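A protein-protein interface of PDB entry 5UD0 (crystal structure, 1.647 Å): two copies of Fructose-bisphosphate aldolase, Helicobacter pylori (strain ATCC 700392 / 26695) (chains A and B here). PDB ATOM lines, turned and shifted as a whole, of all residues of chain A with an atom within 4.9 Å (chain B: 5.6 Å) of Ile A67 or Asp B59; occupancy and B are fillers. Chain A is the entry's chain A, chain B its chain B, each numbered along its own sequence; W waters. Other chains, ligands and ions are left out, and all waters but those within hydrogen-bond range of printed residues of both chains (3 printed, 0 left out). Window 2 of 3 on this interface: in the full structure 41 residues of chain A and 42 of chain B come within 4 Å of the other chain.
Gly A63 touches Ile B67 (CA to CD1, 3.7 Å). Met B60 touches Met A64 (CE to O, 3.7 Å). Ile A67 touches Asp B59. CG2 of Ile A67 touches CE of Met B60 (3.6 Å). CD1 of Ile A67 touches CA of Gly B63 (3.7 Å). Met B60 touches Met A68. Gly B57 touches Arg A71 (CA to NH2, 3.5 Å). Met B60 touches Arg A71 (CB to NH2, 3.6 Å).
NH2 of Arg A71 lies within hydrogen-bond range of O of Met B56 (2.8 Å). The side-chain carboxylate (OD2) of Asp B59 is in salt-bridge range of the guanidinium group (NH2) of Arg A71 (2.9 Å).
Hydrophobic or aromatic side chains of chain A within 4 Å of the printed part of chain B: Met A64, Ile A67 and Met A68. Along chain A the printed residues that touch a printed residue of chain B span positions 63 to 71. Printed residues of chain B that touch a printed residue of chain A: Met B56, Gly B57, Asp B59, Met B60, Gly B63 and Ile B67. Hydrophobic or aromatic side chains of chain B within 4 Å of the printed part of chain A: Met B60 and Ile B67. Among the printed residues, 10 pairs touch across the chains. Among the printed residues, Asp or Glu carboxylates within 4 Å of a Lys or Arg side-chain nitrogen of the other chain: Arg A71 with Asp B59.
The side-chain sulfur (SD) of Met A68 is in hydrogen-bond range of the guanidinium group (NH1) of Arg A71.
Of the printed residues of chain B, Met A64 touches Met B60 (3.7 Å). Ile A67 touches just these residues of chain B: Asp B59, Met B60 and Gly B63. Ile B58 touches none of the printed residues of chain A. Asp B59 touches just these residues of chain A: Ile A67 (3.6 Å) and Arg A71 (2.9 Å). Of the printed residues of chain A, Gly B63 touches Ile A67 (3.7 Å). The nearest residue of chain B that does not touch Ile A67 is Met B64 (4.2 Å). The nearest printed residue of chain B that does not touch Arg A71 is Ile B58 (5.2 Å).
Water W3 bridges OD1 of Asp B59 (2.7 Å) and O of Ile A67 (2.9 Å). Water W2 bridges the side-chain carboxylate of Asp B59 and the guanidinium group of Arg A71. Water W1 bridges O of Met B56 (3.1 Å) and NH1 of Arg A71 (3.2 Å).
Gly A63 touches Ile B67, and with the chains exchanged Ile A67 touches Gly B63. Positions printed for both chains: 63, 64 and 67. Of the 10 pairs that touch across the chains among the printed residues, 2 have their exchanged pair printed and touching as well.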
ATOM      1  N   GLY A  63       0.721   9.505   0.552  1.00  0.00           N
ATOM      2  CA  GLY A  63       1.877   9.324   1.425  1.00  0.00           C
ATOM      3  C   GLY A  63       2.016   7.918   1.975  1.00  0.00           C
ATOM      4  O   GLY A  63       3.122   7.357   2.008  1.00  0.00           O
ATOM      5  N   MET A  64       0.914   7.332   2.472  1.00  0.00           N
ATOM      6  CA  MET A  64       1.015   5.976   2.999  1.00  0.00           C
ATOM      7  C   MET A  64       1.408   4.998   1.911  1.00  0.00           C
ATOM      8  O   MET A  64       2.250   4.121   2.136  1.00  0.00           O
ATOM      9  CB  MET A  64      -0.293   5.534   3.654  1.00  0.00           C
ATOM     10  CG  MET A  64      -0.596   6.222   4.962  1.00  0.00           C
ATOM     11  SD  MET A  64      -1.892   5.392   5.888  1.00  0.00           S
ATOM     12  CE  MET A  64      -3.235   5.443   4.691  1.00  0.00           C
ATOM     13  N   VAL A  65       0.835   5.147   0.715  1.00  0.00           N
ATOM     14  CA  VAL A  65       1.160   4.236  -0.375  1.00  0.00           C
ATOM     15  C   VAL A  65       2.626   4.361  -0.762  1.00  0.00           C
ATOM     16  O   VAL A  65       3.299   3.352  -1.022  1.00  0.00           O
ATOM     17  CB  VAL A  65       0.236   4.483  -1.572  1.00  0.00           C
ATOM     18  CG1 VAL A  65       0.751   3.713  -2.791  1.00  0.00           C
ATOM     19  CG2 VAL A  65      -1.137   4.064  -1.210  1.00  0.00           C
ATOM     20  N   LYS A  66       3.155   5.589  -0.789  1.00  0.00           N
ATOM     21  CA  LYS A  66       4.578   5.775  -1.090  1.00  0.00           C
ATOM     22  C   LYS A  66       5.466   5.101  -0.052  1.00  0.00           C
ATOM     23  O   LYS A  66       6.468   4.461  -0.403  1.00  0.00           O
ATOM     24  CB  LYS A  66       4.907   7.259  -1.213  1.00  0.00           C
ATOM     25  CG  LYS A  66       4.430   7.833  -2.545  1.00  0.00           C
ATOM     26  CD  LYS A  66       4.817   9.281  -2.701  1.00  0.00           C
ATOM     27  CE  LYS A  66       4.362   9.807  -4.050  1.00  0.00           C
ATOM     28  NZ  LYS A  66       4.753  11.230  -4.257  1.00  0.00           N
ATOM     29  N   ILE A  67       5.099   5.190   1.228  1.00  0.00           N
ATOM     30  CA  ILE A  67       5.850   4.485   2.259  1.00  0.00           C
ATOM     31  C   ILE A  67       5.830   2.988   1.996  1.00  0.00           C
ATOM     32  O   ILE A  67       6.856   2.305   2.106  1.00  0.00           O
ATOM     33  CB  ILE A  67       5.292   4.812   3.654  1.00  0.00           C
ATOM     34  CG1 ILE A  67       5.625   6.262   4.037  1.00  0.00           C
ATOM     35  CG2 ILE A  67       5.875   3.838   4.681  1.00  0.00           C
ATOM     36  CD1 ILE A  67       4.747   6.787   5.080  1.00  0.00           C
ATOM     37  N   MET A  68       4.651   2.446   1.689  1.00  0.00           N
ATOM     38  CA  MET A  68       4.542   1.006   1.505  1.00  0.00           C
ATOM     39  C   MET A  68       5.324   0.540   0.277  1.00  0.00           C
ATOM     40  O   MET A  68       5.944  -0.529   0.311  1.00  0.00           O
ATOM     41  CB  MET A  68       3.066   0.595   1.409  1.00  0.00           C
ATOM     42  CG  MET A  68       2.225   0.786   2.708  1.00  0.00           C
ATOM     43  SD  MET A  68       2.875  -0.132   4.146  1.00  0.00           S
ATOM     44  CE  MET A  68       2.803  -1.790   3.450  1.00  0.00           C
ATOM     45  N   CYS A  69       5.296   1.322  -0.808  1.00  0.00           N
ATOM     46  CA  CYS A  69       6.110   1.005  -1.982  1.00  0.00           C
ATOM     47  C   CYS A  69       7.587   0.903  -1.624  1.00  0.00           C
ATOM     48  O   CYS A  69       8.289  -0.005  -2.092  1.00  0.00           O
ATOM     49  CB  CYS A  69       5.901   2.055  -3.065  1.00  0.00           C
ATOM     50  SG  CYS A  69       4.368   1.774  -3.887  1.00  0.00           S
ATOM     51  N   GLU A  70       8.082   1.840  -0.811  1.00  0.00           N
ATOM     52  CA  GLU A  70       9.472   1.798  -0.368  1.00  0.00           C
ATOM     53  C   GLU A  70       9.739   0.618   0.551  1.00  0.00           C
ATOM     54  O   GLU A  70      10.863   0.114   0.607  1.00  0.00           O
ATOM     55  CB  GLU A  70       9.843   3.113   0.326  1.00  0.00           C
ATOM     56  CG  GLU A  70       9.839   4.288  -0.621  1.00  0.00           C
ATOM     57  CD  GLU A  70      10.575   5.488  -0.061  1.00  0.00           C
ATOM     58  OE1 GLU A  70      11.372   6.097  -0.805  1.00  0.00           O
ATOM     59  OE2 GLU A  70      10.363   5.817   1.126  1.00  0.00           O
ATOM     60  N   ARG A  71       8.725   0.153   1.271  1.00  0.00           N
ATOM     61  CA  ARG A  71       8.897  -1.045   2.070  1.00  0.00           C
ATOM     62  C   ARG A  71       9.005  -2.304   1.212  1.00  0.00           C
ATOM     63  O   ARG A  71       9.685  -3.259   1.608  1.00  0.00           O
ATOM     64  CB  ARG A  71       7.729  -1.158   3.039  1.00  0.00           C
ATOM     65  CG  ARG A  71       7.868  -2.193   4.079  1.00  0.00           C
ATOM     66  CD  ARG A  71       6.611  -2.236   4.908  1.00  0.00           C
ATOM     67  NE  ARG A  71       6.502  -1.142   5.879  1.00  0.00           N
ATOM     68  CZ  ARG A  71       5.526  -1.076   6.778  1.00  0.00           C
ATOM     69  NH1 ARG A  71       4.570  -2.005   6.792  1.00  0.00           N
ATOM     70  NH2 ARG A  71       5.484  -0.066   7.640  1.00  0.00           N
ATOM     71  N   MET B  56       3.021  -0.811  13.321  1.00  0.00           N
ATOM     72  CA  MET B  56       2.983   0.069  12.139  1.00  0.00           C
ATOM     73  C   MET B  56       4.168  -0.147  11.192  1.00  0.00           C
ATOM     74  O   MET B  56       4.032   0.028   9.974  1.00  0.00           O
ATOM     75  CB  MET B  56       2.961   1.550  12.567  1.00  0.00           C
ATOM     76  CG  MET B  56       1.617   2.041  13.047  1.00  0.00           C
ATOM     77  SD  MET B  56       1.766   3.747  13.625  1.00  0.00           S
ATOM     78  CE  MET B  56       2.594   3.494  15.181  1.00  0.00           C
ATOM     79  N   GLY B  57       5.334  -0.496  11.716  1.00  0.00           N
ATOM     80  CA  GLY B  57       6.575  -0.273  11.005  1.00  0.00           C
ATOM     81  C   GLY B  57       7.098   1.108  11.338  1.00  0.00           C
ATOM     82  O   GLY B  57       6.337   2.077  11.256  1.00  0.00           O
ATOM     83  N   ILE B  58       8.355   1.218  11.786  1.00  0.00           N
ATOM     84  CA  ILE B  58       8.857   2.532  12.188  1.00  0.00           C
ATOM     85  C   ILE B  58       8.803   3.528  11.031  1.00  0.00           C
ATOM     86  O   ILE B  58       8.612   4.734  11.246  1.00  0.00           O
ATOM     87  CB  ILE B  58      10.279   2.401  12.774  1.00  0.00           C
ATOM     88  CG1 ILE B  58      10.604   3.638  13.618  1.00  0.00           C
ATOM     89  CG2 ILE B  58      11.317   2.160  11.674  1.00  0.00           C
ATOM     90  CD1 ILE B  58      11.836   3.466  14.473  1.00  0.00           C
ATOM     91  N   ASP B  59       8.984   3.047   9.799  1.00  0.00           N
ATOM     92  CA  ASP B  59       8.888   3.887   8.605  1.00  0.00           C
ATOM     93  C   ASP B  59       7.496   4.477   8.448  1.00  0.00           C
ATOM     94  O   ASP B  59       7.352   5.633   8.052  1.00  0.00           O
ATOM     95  CB  ASP B  59       9.273   3.071   7.361  1.00  0.00           C
ATOM     96  CG  ASP B  59       8.449   1.803   7.198  1.00  0.00           C
ATOM     97  OD1 ASP B  59       8.171   1.438   6.037  1.00  0.00           O
ATOM     98  OD2 ASP B  59       8.080   1.155   8.206  1.00  0.00           O
ATOM     99  N   MET B  60       6.460   3.724   8.813  1.00  0.00           N
ATOM    100  CA  MET B  60       5.110   4.254   8.707  1.00  0.00           C
ATOM    101  C   MET B  60       4.806   5.161   9.887  1.00  0.00           C
ATOM    102  O   MET B  60       4.113   6.175   9.740  1.00  0.00           O
ATOM    103  CB  MET B  60       4.089   3.118   8.631  1.00  0.00           C
ATOM    104  CG  MET B  60       2.657   3.586   8.427  1.00  0.00           C
ATOM    105  SD  MET B  60       2.335   4.408   6.830  1.00  0.00           S
ATOM    106  CE  MET B  60       2.562   3.033   5.672  1.00  0.00           C
ATOM    107  N   ALA B  61       5.301   4.803  11.069  1.00  0.00           N
ATOM    108  CA  ALA B  61       5.047   5.651  12.225  1.00  0.00           C
ATOM    109  C   ALA B  61       5.629   7.036  12.008  1.00  0.00           C
ATOM    110  O   ALA B  61       4.942   8.050  12.191  1.00  0.00           O
ATOM    111  CB  ALA B  61       5.622   5.002  13.480  1.00  0.00           C
ATOM    112  N   VAL B  62       6.883   7.107  11.563  1.00  0.00           N
ATOM    113  CA  VAL B  62       7.482   8.419  11.323  1.00  0.00           C
ATOM    114  C   VAL B  62       6.838   9.070  10.100  1.00  0.00           C
ATOM    115  O   VAL B  62       6.526  10.274  10.107  1.00  0.00           O
ATOM    116  CB  VAL B  62       9.008   8.292  11.164  1.00  0.00           C
ATOM    117  CG1 VAL B  62       9.608   9.629  10.738  1.00  0.00           C
ATOM    118  CG2 VAL B  62       9.659   7.822  12.479  1.00  0.00           C
ATOM    119  N   GLY B  63       6.581   8.282   9.057  1.00  0.00           N
ATOM    120  CA  GLY B  63       6.070   8.844   7.814  1.00  0.00           C
ATOM    121  C   GLY B  63       4.704   9.482   7.975  1.00  0.00           C
ATOM    122  O   GLY B  63       4.445  10.573   7.450  1.00  0.00           O
ATOM    123  N   MET B  64       3.796   8.806   8.684  1.00  0.00           N
ATOM    124  CA  MET B  64       2.476   9.372   8.913  1.00  0.00           C
ATOM    125  C   MET B  64       2.574  10.666   9.703  1.00  0.00           C
ATOM    126  O   MET B  64       1.898  11.648   9.382  1.00  0.00           O
ATOM    127  CB  MET B  64       1.569   8.376   9.642  1.00  0.00           C
ATOM    128  CG  MET B  64       1.095   7.212   8.754  1.00  0.00           C
ATOM    129  SD  MET B  64      -0.299   6.342   9.461  1.00  0.00           S
ATOM    130  CE  MET B  64       0.399   5.760  10.995  1.00  0.00           C
ATOM    131  N   ILE B  67       3.709  13.517   7.488  1.00  0.00           N
ATOM    132  CA  ILE B  67       2.591  13.969   6.667  1.00  0.00           C
ATOM    133  C   ILE B  67       1.665  14.876   7.482  1.00  0.00           C
ATOM    134  O   ILE B  67       1.224  15.940   7.014  1.00  0.00           O
ATOM    135  CB  ILE B  67       1.836  12.764   6.098  1.00  0.00           C
ATOM    136  CG1 ILE B  67       2.713  12.019   5.079  1.00  0.00           C
ATOM    137  CG2 ILE B  67       0.542  13.234   5.433  1.00  0.00           C
ATOM    138  CD1 ILE B  67       2.286  10.585   4.843  1.00  0.00           C
HETATM  139  O   HOH W   1       3.543  -3.024   9.592  1.00  0.00           O
HETATM  140  O   HOH W   2       8.647  -1.761   8.438  1.00  0.00           O
HETATM  141  O   HOH W   3       9.127   2.538   3.821  1.00  0.00           O
